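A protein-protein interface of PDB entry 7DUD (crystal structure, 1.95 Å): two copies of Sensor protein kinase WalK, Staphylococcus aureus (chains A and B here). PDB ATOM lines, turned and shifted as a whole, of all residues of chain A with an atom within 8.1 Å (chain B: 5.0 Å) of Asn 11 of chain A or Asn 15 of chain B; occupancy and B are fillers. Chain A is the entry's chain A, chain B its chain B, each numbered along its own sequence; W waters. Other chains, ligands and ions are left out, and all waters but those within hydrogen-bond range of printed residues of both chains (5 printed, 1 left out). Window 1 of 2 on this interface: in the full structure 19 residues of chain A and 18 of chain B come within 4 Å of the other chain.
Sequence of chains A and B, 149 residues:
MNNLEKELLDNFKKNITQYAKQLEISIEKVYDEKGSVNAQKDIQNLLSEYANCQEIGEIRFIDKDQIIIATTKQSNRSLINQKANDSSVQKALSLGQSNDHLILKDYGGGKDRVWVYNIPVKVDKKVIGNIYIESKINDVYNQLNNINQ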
ATOM      1  N   LEU A   4      11.801 -11.114  17.282  1.00  0.00           N
ATOM      2  CA  LEU A   4      11.844 -12.535  17.628  1.00  0.00           C
ATOM      3  C   LEU A   4      12.159 -13.391  16.410  1.00  0.00           C
ATOM      4  O   LEU A   4      12.917 -14.362  16.510  1.00  0.00           O
ATOM      5  CB  LEU A   4      10.524 -12.993  18.243  1.00  0.00           C
ATOM      6  CG  LEU A   4      10.542 -14.455  18.720  1.00  0.00           C
ATOM      7  CD1 LEU A   4      11.628 -14.627  19.771  1.00  0.00           C
ATOM      8  CD2 LEU A   4       9.198 -14.895  19.269  1.00  0.00           C
ATOM      9  N   GLU A   5      11.551 -13.075  15.259  1.00  0.00           N
ATOM     10  CA  GLU A   5      11.843 -13.829  14.037  1.00  0.00           C
ATOM     11  C   GLU A   5      13.340 -13.818  13.722  1.00  0.00           C
ATOM     12  O   GLU A   5      13.950 -14.876  13.503  1.00  0.00           O
ATOM     13  CB  GLU A   5      11.036 -13.264  12.859  1.00  0.00           C
ATOM     14  CG  GLU A   5      11.092 -14.130  11.607  1.00  0.00           C
ATOM     15  CD  GLU A   5      10.501 -13.470  10.361  1.00  0.00           C
ATOM     16  OE1 GLU A   5       9.598 -12.626  10.509  1.00  0.00           O
ATOM     17  OE2 GLU A   5      10.924 -13.812   9.231  1.00  0.00           O
ATOM     18  N   LYS A   6      13.941 -12.621  13.675  1.00  0.00           N
ATOM     19  CA  LYS A   6      15.375 -12.521  13.395  1.00  0.00           C
ATOM     20  C   LYS A   6      16.180 -13.351  14.377  1.00  0.00           C
ATOM     21  O   LYS A   6      17.107 -14.073  13.990  1.00  0.00           O
ATOM     22  CB  LYS A   6      15.848 -11.067  13.472  1.00  0.00           C
ATOM     23  CG  LYS A   6      17.365 -10.942  13.213  1.00  0.00           C
ATOM     24  CD  LYS A   6      17.834  -9.497  13.261  1.00  0.00           C
ATOM     25  CE  LYS A   6      19.291  -9.442  13.723  1.00  0.00           C
ATOM     26  NZ  LYS A   6      20.144 -10.405  12.925  1.00  0.00           N
ATOM     27  N   GLU A   7      15.843 -13.235  15.664  1.00  0.00           N
ATOM     28  CA  GLU A   7      16.558 -13.934  16.725  1.00  0.00           C
ATOM     29  C   GLU A   7      16.508 -15.449  16.541  1.00  0.00           C
ATOM     30  O   GLU A   7      17.543 -16.124  16.561  1.00  0.00           O
ATOM     31  CB  GLU A   7      15.953 -13.514  18.069  1.00  0.00           C
ATOM     32  CG  GLU A   7      16.340 -12.082  18.472  1.00  0.00           C
ATOM     33  CD  GLU A   7      15.655 -11.627  19.733  1.00  0.00           C
ATOM     34  OE1 GLU A   7      14.663 -12.287  20.125  1.00  0.00           O
ATOM     35  OE2 GLU A   7      16.131 -10.639  20.359  1.00  0.00           O
ATOM     36  N   LEU A   8      15.307 -16.001  16.382  1.00  0.00           N
ATOM     37  CA  LEU A   8      15.173 -17.453  16.270  1.00  0.00           C
ATOM     38  C   LEU A   8      15.841 -17.984  15.003  1.00  0.00           C
ATOM     39  O   LEU A   8      16.459 -19.058  15.029  1.00  0.00           O
ATOM     40  CB  LEU A   8      13.692 -17.852  16.344  1.00  0.00           C
ATOM     41  CG  LEU A   8      12.998 -17.576  17.697  1.00  0.00           C
ATOM     42  CD1 LEU A   8      11.718 -18.371  17.795  1.00  0.00           C
ATOM     43  CD2 LEU A   8      13.906 -17.886  18.902  1.00  0.00           C
ATOM     44  N   LEU A   9      15.759 -17.226  13.895  1.00  0.00           N
ATOM     45  CA  LEU A   9      16.416 -17.636  12.651  1.00  0.00           C
ATOM     46  C   LEU A   9      17.938 -17.602  12.780  1.00  0.00           C
ATOM     47  O   LEU A   9      18.634 -18.513  12.292  1.00  0.00           O
ATOM     48  CB  LEU A   9      15.958 -16.746  11.487  1.00  0.00           C
ATOM     49  CG  LEU A   9      14.505 -16.963  11.039  1.00  0.00           C
ATOM     50  CD1 LEU A   9      14.075 -15.905   9.994  1.00  0.00           C
ATOM     51  CD2 LEU A   9      14.337 -18.383  10.528  1.00  0.00           C
ATOM     52  N   ASP A  10      18.479 -16.553  13.415  1.00  0.00           N
ATOM     53  CA  ASP A  10      19.920 -16.514  13.671  1.00  0.00           C
ATOM     54  C   ASP A  10      20.353 -17.672  14.543  1.00  0.00           C
ATOM     55  O   ASP A  10      21.399 -18.267  14.293  1.00  0.00           O
ATOM     56  CB  ASP A  10      20.355 -15.199  14.335  1.00  0.00           C
ATOM     57  CG  ASP A  10      20.238 -13.991  13.416  1.00  0.00           C
ATOM     58  OD1 ASP A  10      20.204 -14.172  12.174  1.00  0.00           O
ATOM     59  OD2 ASP A  10      20.178 -12.858  13.947  1.00  0.00           O
ATOM     60  N   ASN A  11      19.594 -17.963  15.608  1.00  0.00           N
ATOM     61  CA  ASN A  11      19.940 -19.087  16.479  1.00  0.00           C
ATOM     62  C   ASN A  11      19.959 -20.408  15.715  1.00  0.00           C
ATOM     63  O   ASN A  11      20.855 -21.246  15.915  1.00  0.00           O
ATOM     64  CB  ASN A  11      18.948 -19.196  17.643  1.00  0.00           C
ATOM     65  CG  ASN A  11      18.889 -17.945  18.494  1.00  0.00           C
ATOM     66  OD1 ASN A  11      19.811 -17.135  18.501  1.00  0.00           O
ATOM     67  ND2 ASN A  11      17.805 -17.797  19.237  1.00  0.00           N
ATOM     68  N   PHE A  12      18.964 -20.626  14.855  1.00  0.00           N
ATOM     69  CA  PHE A  12      18.904 -21.866  14.086  1.00  0.00           C
ATOM     70  C   PHE A  12      20.126 -21.996  13.196  1.00  0.00           C
ATOM     71  O   PHE A  12      20.767 -23.054  13.115  1.00  0.00           O
ATOM     72  CB  PHE A  12      17.623 -21.877  13.243  1.00  0.00           C
ATOM     73  CG  PHE A  12      17.449 -23.115  12.416  1.00  0.00           C
ATOM     74  CD1 PHE A  12      17.997 -23.193  11.148  1.00  0.00           C
ATOM     75  CD2 PHE A  12      16.729 -24.198  12.903  1.00  0.00           C
ATOM     76  CE1 PHE A  12      17.848 -24.327  10.374  1.00  0.00           C
ATOM     77  CE2 PHE A  12      16.553 -25.337  12.123  1.00  0.00           C
ATOM     78  CZ  PHE A  12      17.134 -25.403  10.865  1.00  0.00           C
ATOM     79  N   LYS A  13      20.459 -20.909  12.511  1.00  0.00           N
ATOM     80  CA  LYS A  13      21.576 -20.939  11.581  1.00  0.00           C
ATOM     81  C   LYS A  13      22.900 -21.107  12.321  1.00  0.00           C
ATOM     82  O   LYS A  13      23.811 -21.803  11.847  1.00  0.00           O
ATOM     83  CB  LYS A  13      21.543 -19.642  10.775  1.00  0.00           C
ATOM     84  CG  LYS A  13      20.418 -19.561   9.731  1.00  0.00           C
ATOM     85  CD  LYS A  13      20.444 -18.157   9.127  1.00  0.00           C
ATOM     86  CE  LYS A  13      19.371 -17.995   8.105  1.00  0.00           C
ATOM     87  NZ  LYS A  13      19.474 -16.659   7.450  1.00  0.00           N
ATOM     88  N   LYS A  14      23.019 -20.503  13.506  1.00  0.00           N
ATOM     89  CA  LYS A  14      24.223 -20.690  14.312  1.00  0.00           C
ATOM     90  C   LYS A  14      24.366 -22.151  14.733  1.00  0.00           C
ATOM     91  O   LYS A  14      25.449 -22.754  14.610  1.00  0.00           O
ATOM     92  CB  LYS A  14      24.167 -19.738  15.523  1.00  0.00           C
ATOM     93  CG  LYS A  14      25.503 -19.521  16.225  1.00  0.00           C
ATOM     94  CD  LYS A  14      25.358 -18.533  17.385  1.00  0.00           C
ATOM     95  CE  LYS A  14      26.733 -18.319  18.031  1.00  0.00           C
ATOM     96  NZ  LYS A  14      26.743 -17.374  19.160  1.00  0.00           N
ATOM     97  N   ASN A  15      23.271 -22.756  15.210  1.00  0.00           N
ATOM     98  CA  ASN A  15      23.289 -24.174  15.557  1.00  0.00           C
ATOM     99  C   ASN A  15      23.855 -25.004  14.413  1.00  0.00           C
ATOM    100  O   ASN A  15      24.791 -25.799  14.589  1.00  0.00           O
ATOM    101  CB  ASN A  15      21.867 -24.667  15.885  1.00  0.00           C
ATOM    102  CG  ASN A  15      21.482 -24.449  17.328  1.00  0.00           C
ATOM    103  OD1 ASN A  15      22.294 -24.648  18.241  1.00  0.00           O
ATOM    104  ND2 ASN A  15      20.224 -24.073  17.549  1.00  0.00           N
ATOM    105  N   ILE A  16      23.274 -24.818  13.220  1.00  0.00           N
ATOM    106  CA  ILE A  16      23.678 -25.601  12.049  1.00  0.00           C
ATOM    107  C   ILE A  16      25.156 -25.369  11.714  1.00  0.00           C
ATOM    108  O   ILE A  16      25.896 -26.313  11.418  1.00  0.00           O
ATOM    109  CB  ILE A  16      22.789 -25.260  10.833  1.00  0.00           C
ATOM    110  CG1 ILE A  16      21.315 -25.576  11.087  1.00  0.00           C
ATOM    111  CG2 ILE A  16      23.331 -25.954   9.566  1.00  0.00           C
ATOM    112  CD1 ILE A  16      21.030 -27.021  11.280  1.00  0.00           C
ATOM    113  N   THR A  17      25.605 -24.115  11.724  1.00  0.00           N
ATOM    114  CA  THR A  17      26.979 -23.852  11.284  1.00  0.00           C
ATOM    115  C   THR A  17      28.020 -24.355  12.280  1.00  0.00           C
ATOM    116  O   THR A  17      29.073 -24.849  11.866  1.00  0.00           O
ATOM    117  CB  THR A  17      27.179 -22.374  11.010  1.00  0.00           C
ATOM    118  OG1 THR A  17      26.960 -21.623  12.212  1.00  0.00           O
ATOM    119  CG2 THR A  17      26.196 -21.940   9.940  1.00  0.00           C
ATOM    120  N   GLN A  18      27.764 -24.249  13.586  1.00  0.00           N
ATOM    121  CA  GLN A  18      28.739 -24.761  14.557  1.00  0.00           C
ATOM    122  C   GLN A  18      28.816 -26.285  14.498  1.00  0.00           C
ATOM    123  O   GLN A  18      29.912 -26.875  14.497  1.00  0.00           O
ATOM    124  CB  GLN A  18      28.366 -24.294  15.960  1.00  0.00           C
ATOM    125  CG  GLN A  18      28.435 -22.792  16.150  1.00  0.00           C
ATOM    126  CD  GLN A  18      27.866 -22.330  17.482  1.00  0.00           C
ATOM    127  OE1 GLN A  18      26.847 -22.855  17.965  1.00  0.00           O
ATOM    128  NE2 GLN A  18      28.516 -21.333  18.084  1.00  0.00           N
ATOM    129  N   TRP A 115      17.021 -24.225   4.470  1.00  0.00           N
ATOM    130  CA  TRP A 115      18.223 -23.407   4.473  1.00  0.00           C
ATOM    131  C   TRP A 115      19.379 -24.277   3.997  1.00  0.00           C
ATOM    132  O   TRP A 115      19.635 -25.346   4.560  1.00  0.00           O
ATOM    133  CB  TRP A 115      18.474 -22.813   5.855  1.00  0.00           C
ATOM    134  CG  TRP A 115      19.586 -21.784   5.876  1.00  0.00           C
ATOM    135  CD1 TRP A 115      19.656 -20.623   5.168  1.00  0.00           C
ATOM    136  CD2 TRP A 115      20.768 -21.851   6.666  1.00  0.00           C
ATOM    137  NE1 TRP A 115      20.830 -19.951   5.468  1.00  0.00           N
ATOM    138  CE2 TRP A 115      21.526 -20.690   6.392  1.00  0.00           C
ATOM    139  CE3 TRP A 115      21.258 -22.779   7.599  1.00  0.00           C
ATOM    140  CZ2 TRP A 115      22.751 -20.443   7.003  1.00  0.00           C
ATOM    141  CZ3 TRP A 115      22.492 -22.533   8.200  1.00  0.00           C
ATOM    142  CH2 TRP A 115      23.214 -21.366   7.906  1.00  0.00           C
ATOM    143  N   ILE A 137      14.771 -25.205   8.206  1.00  0.00           N
ATOM    144  CA  ILE A 137      14.537 -23.903   8.830  1.00  0.00           C
ATOM    145  C   ILE A 137      13.044 -23.575   8.880  1.00  0.00           C
ATOM    146  O   ILE A 137      12.613 -22.743   9.694  1.00  0.00           O
ATOM    147  CB  ILE A 137      15.348 -22.819   8.102  1.00  0.00           C
ATOM    148  CG1 ILE A 137      15.467 -21.582   9.006  1.00  0.00           C
ATOM    149  CG2 ILE A 137      14.723 -22.526   6.738  1.00  0.00           C
ATOM    150  CD1 ILE A 137      16.735 -20.758   8.805  1.00  0.00           C
ATOM    151  N   VAL A 140      11.378 -23.188  12.289  1.00  0.00           N
ATOM    152  CA  VAL A 140      11.325 -21.882  12.935  1.00  0.00           C
ATOM    153  C   VAL A 140      10.154 -21.075  12.393  1.00  0.00           C
ATOM    154  O   VAL A 140       9.381 -20.482  13.156  1.00  0.00           O
ATOM    155  CB  VAL A 140      12.653 -21.120  12.769  1.00  0.00           C
ATOM    156  CG1 VAL A 140      12.465 -19.722  13.277  1.00  0.00           C
ATOM    157  CG2 VAL A 140      13.749 -21.815  13.555  1.00  0.00           C
ATOM    158  N   ASN B  11      23.092 -21.792  22.660  1.00  0.00           N
ATOM    159  CA  ASN B  11      22.061 -21.555  21.658  1.00  0.00           C
ATOM    160  C   ASN B  11      20.695 -22.039  22.129  1.00  0.00           C
ATOM    161  O   ASN B  11      19.683 -21.361  21.934  1.00  0.00           O
ATOM    162  CB  ASN B  11      22.413 -22.277  20.365  1.00  0.00           C
ATOM    163  CG  ASN B  11      23.710 -21.798  19.756  1.00  0.00           C
ATOM    164  OD1 ASN B  11      24.269 -20.773  20.170  1.00  0.00           O
ATOM    165  ND2 ASN B  11      24.214 -22.560  18.776  1.00  0.00           N
ATOM    166  N   PHE B  12      20.641 -23.235  22.703  1.00  0.00           N
ATOM    167  CA  PHE B  12      19.366 -23.735  23.208  1.00  0.00           C
ATOM    168  C   PHE B  12      18.784 -22.788  24.246  1.00  0.00           C
ATOM    169  O   PHE B  12      17.603 -22.405  24.180  1.00  0.00           O
ATOM    170  CB  PHE B  12      19.557 -25.146  23.783  1.00  0.00           C
ATOM    171  CG  PHE B  12      18.310 -25.734  24.387  1.00  0.00           C
ATOM    172  CD1 PHE B  12      17.952 -25.446  25.690  1.00  0.00           C
ATOM    173  CD2 PHE B  12      17.553 -26.667  23.668  1.00  0.00           C
ATOM    174  CE1 PHE B  12      16.823 -26.023  26.260  1.00  0.00           C
ATOM    175  CE2 PHE B  12      16.401 -27.237  24.218  1.00  0.00           C
ATOM    176  CZ  PHE B  12      16.037 -26.916  25.514  1.00  0.00           C
ATOM    177  N   LYS B  13      19.600 -22.393  25.221  1.00  0.00           N
ATOM    178  CA  LYS B  13      19.058 -21.520  26.256  1.00  0.00           C
ATOM    179  C   LYS B  13      18.650 -20.170  25.680  1.00  0.00           C
ATOM    180  O   LYS B  13      17.676 -19.574  26.143  1.00  0.00           O
ATOM    181  CB  LYS B  13      20.077 -21.354  27.374  1.00  0.00           C
ATOM    182  CG  LYS B  13      20.388 -22.672  28.099  1.00  0.00           C
ATOM    183  CD  LYS B  13      21.527 -22.478  29.085  1.00  0.00           C
ATOM    184  CE  LYS B  13      21.834 -23.743  29.894  1.00  0.00           C
ATOM    185  NZ  LYS B  13      22.907 -23.440  30.922  1.00  0.00           N
ATOM    186  N   LYS B  14      19.369 -19.674  24.672  1.00  0.00           N
ATOM    187  CA  LYS B  14      18.982 -18.412  24.034  1.00  0.00           C
ATOM    188  C   LYS B  14      17.618 -18.522  23.344  1.00  0.00           C
ATOM    189  O   LYS B  14      16.782 -17.619  23.486  1.00  0.00           O
ATOM    190  CB  LYS B  14      20.069 -17.986  23.044  1.00  0.00           C
ATOM    191  CG  LYS B  14      20.091 -16.459  22.779  1.00  0.00           C
ATOM    192  CD  LYS B  14      21.415 -16.030  22.116  1.00  0.00           C
ATOM    193  CE  LYS B  14      21.345 -14.601  21.620  1.00  0.00           C
ATOM    194  NZ  LYS B  14      22.378 -14.304  20.581  1.00  0.00           N
ATOM    195  N   ASN B  15      17.383 -19.610  22.593  1.00  0.00           N
ATOM    196  CA  ASN B  15      16.065 -19.887  22.013  1.00  0.00           C
ATOM    197  C   ASN B  15      14.972 -19.813  23.065  1.00  0.00           C
ATOM    198  O   ASN B  15      13.955 -19.132  22.876  1.00  0.00           O
ATOM    199  CB  ASN B  15      16.003 -21.296  21.385  1.00  0.00           C
ATOM    200  CG  ASN B  15      16.602 -21.384  19.981  1.00  0.00           C
ATOM    201  OD1 ASN B  15      16.523 -20.445  19.179  1.00  0.00           O
ATOM    202  ND2 ASN B  15      17.146 -22.578  19.651  1.00  0.00           N
ATOM    203  N   ILE B  16      15.143 -20.573  24.163  1.00  0.00           N
ATOM    204  CA  ILE B  16      14.110 -20.608  25.210  1.00  0.00           C
ATOM    205  C   ILE B  16      13.907 -19.231  25.834  1.00  0.00           C
ATOM    206  O   ILE B  16      12.767 -18.811  26.084  1.00  0.00           O
ATOM    207  CB  ILE B  16      14.441 -21.660  26.287  1.00  0.00           C
ATOM    208  CG1 ILE B  16      14.426 -23.078  25.713  1.00  0.00           C
ATOM    209  CG2 ILE B  16      13.447 -21.568  27.467  1.00  0.00           C
ATOM    210  CD1 ILE B  16      13.101 -23.421  24.971  1.00  0.00           C
ATOM    211  N   THR B  17      14.997 -18.509  26.127  1.00  0.00           N
ATOM    212  CA  THR B  17      14.803 -17.244  26.835  1.00  0.00           C
ATOM    213  C   THR B  17      14.195 -16.178  25.935  1.00  0.00           C
ATOM    214  O   THR B  17      13.350 -15.405  26.393  1.00  0.00           O
ATOM    215  CB  THR B  17      16.105 -16.734  27.464  1.00  0.00           C
ATOM    216  OG1 THR B  17      17.000 -16.314  26.433  1.00  0.00           O
ATOM    217  CG2 THR B  17      16.759 -17.804  28.309  1.00  0.00           C
ATOM    218  N   GLN B  18      14.584 -16.114  24.650  1.00  0.00           N
ATOM    219  CA  GLN B  18      14.009 -15.093  23.763  1.00  0.00           C
ATOM    220  C   GLN B  18      12.529 -15.356  23.514  1.00  0.00           C
ATOM    221  O   GLN B  18      11.700 -14.419  23.494  1.00  0.00           O
ATOM    222  CB  GLN B  18      14.783 -15.087  22.451  1.00  0.00           C
ATOM    223  CG  GLN B  18      16.225 -14.567  22.638  1.00  0.00           C
ATOM    224  CD  GLN B  18      17.048 -14.638  21.356  1.00  0.00           C
ATOM    225  OE1 GLN B  18      16.908 -15.576  20.556  1.00  0.00           O
ATOM    226  NE2 GLN B  18      17.932 -13.657  21.168  1.00  0.00           N
ATOM    227  N   TYR B  19      12.196 -16.638  23.322  1.00  0.00           N
ATOM    228  CA  TYR B  19      10.814 -17.081  23.179  1.00  0.00           C
ATOM    229  C   TYR B  19       9.996 -16.721  24.416  1.00  0.00           C
ATOM    230  O   TYR B  19       8.890 -16.173  24.311  1.00  0.00           O
ATOM    231  CB  TYR B  19      10.857 -18.599  22.954  1.00  0.00           C
ATOM    232  CG  TYR B  19       9.589 -19.317  22.556  1.00  0.00           C
ATOM    233  CD1 TYR B  19       9.028 -19.126  21.287  1.00  0.00           C
ATOM    234  CD2 TYR B  19       9.008 -20.264  23.400  1.00  0.00           C
ATOM    235  CE1 TYR B  19       7.889 -19.810  20.898  1.00  0.00           C
ATOM    236  CE2 TYR B  19       7.839 -20.971  23.000  1.00  0.00           C
ATOM    237  CZ  TYR B  19       7.301 -20.724  21.743  1.00  0.00           C
ATOM    238  OH  TYR B  19       6.175 -21.392  21.301  1.00  0.00           O
ATOM    239  N   ALA B  20      10.533 -17.036  25.606  1.00  0.00           N
ATOM    240  CA  ALA B  20       9.872 -16.704  26.868  1.00  0.00           C
ATOM    241  C   ALA B  20       9.707 -15.197  27.055  1.00  0.00           C
ATOM    242  O   ALA B  20       8.728 -14.749  27.666  1.00  0.00           O
ATOM    243  CB  ALA B  20      10.660 -17.293  28.046  1.00  0.00           C
HETATM  244  O   HOH W   1      12.707 -11.954  22.541  1.00  0.00           O
HETATM  245  O   HOH W   2      27.249 -20.148  20.627  1.00  0.00           O
HETATM  246  O   HOH W   3      15.741 -21.044  16.573  1.00  0.00           O
HETATM  247  O   HOH W   4      19.387 -14.319  18.667  1.00  0.00           O
HETATM  248  O   HOH W   5      17.100 -23.168  16.845  1.00  0.00           O
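Asn 11 of chain A touches Asn 15 of chain B, and with the chains exchanged Asn 15 of chain A touches Asn 11 of chain B. Asn 11 of chain A touches Gln 18 of chain B, and with the chains exchanged Gln 18 of chain A touches Asn 11 of chain B. Lys 14 of chain A touches Asn 11 of chain B, but with the chains exchanged Asn 11 of chain A does not touch Lys 14 of chain B (4.1 Å). Positions printed for both chains: 11, 12, 13, 14, 15, 16, 17 and 18. Of the 8 pairs that touch across the chains among the printed residues, 4 have their exchanged pair printed and touching as well.
ND2 of Asn 11 of chain A lies within hydrogen-bond range of OD1 of Asn 15 of chain B (2.9 Å). The side-chain amide nitrogen (ND2) of Asn 11 of chain A is in hydrogen-bond range of the side-chain amide oxygen (OE1) of Gln 18 of chain B, at 2.7 Å. OD1 of Asn 15 of chain A is in hydrogen-bond range of ND2 of Asn 11 of chain B (2.9 Å). The side-chain amide nitrogen of Asn 11 of chain B lies within hydrogen-bond range of the side-chain amide oxygen of Gln 18 of chain A.
Among the printed residues, merely in contact across the chains: Leu 4 of chain A with Gln 18 of chain B, Glu 7 of chain A with Gln 18 of chain B, Leu 8 of chain A with Asn 15 of chain B and Lys 14 of chain A with Asn 11 of chain B.
Water W3 lies within hydrogen-bond range of O of Leu 8 of chain A (2.6 Å) and OD1 of Asn 15 of chain B (2.8 Å). Water W1 bridges O of Gln 18 of chain B (2.8 Å) and OE1 of Glu 7 of chain A (3.1 Å). Water W4 lies within hydrogen-bond range of the side-chain amide oxygen of Asn 11 of chain A, the side-chain amide nitrogen of Gln 18 of chain B and the backbone carbonyl oxygen of Glu 7 of chain A. Water W5 bridges the side-chain amide nitrogen of Asn 15 of chain B and the side-chain amide nitrogen of Asn 15 of chain A. Water W2 lies within hydrogen-bond range of the side-chain amide oxygen (OD1) of Asn 11 of chain B, the side-chain amide nitrogen (NE2) of Gln 18 of chain A and the side-chain amino group (NZ) of Lys 14 of chain A.
Printed residues of chain A that touch a printed residue of chain B: Leu 4, Glu 7, Leu 8, Asn 11, Lys 14, Asn 15 and Gln 18. Of the 10 printed residues of chain B, 3 touch a printed residue of chain A. Among the printed residues, no Asp or Glu carboxylate lies within 4 Å of a Lys or Arg side-chain nitrogen of the other chain.
O of Glu 7 of chain A sits close to OD1 of Asn 11 of chain A, 3.2 Å away. O of Asn 11 of chain A lies within hydrogen-bond range of ND2 of Asn 15 of chain A, at 3.3 Å. The side-chain hydroxyl (OG1) of Thr 17 of chain A lies within hydrogen-bond range of the backbone carbonyl oxygen (O) of Lys 14 of chain A.
Asn 11 of chain A touches just these residues of chain B: Asn 15 and Gln 18. Of the printed residues of chain A, Asn 15 of chain B touches Leu 8 and Asn 11. Of the printed residues of chain B, Gln 18 of chain A touches Asn 11 (2.8 Å). Of the printed residues of chain B, Glu 7 of chain A touches Gln 18. Printed residues of chain A within 4 Å of Gln 18 of chain B: Leu 4, Glu 7 and Asn 11. Printed residues of chain A within 4 Å of Asn 11 of chain B: Lys 14, Asn 15 and Gln 18. Of the printed residues of chain B, Leu 8 of chain A touches Asn 15. Tyr 19 of chain B touches none of the printed residues of chain A.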
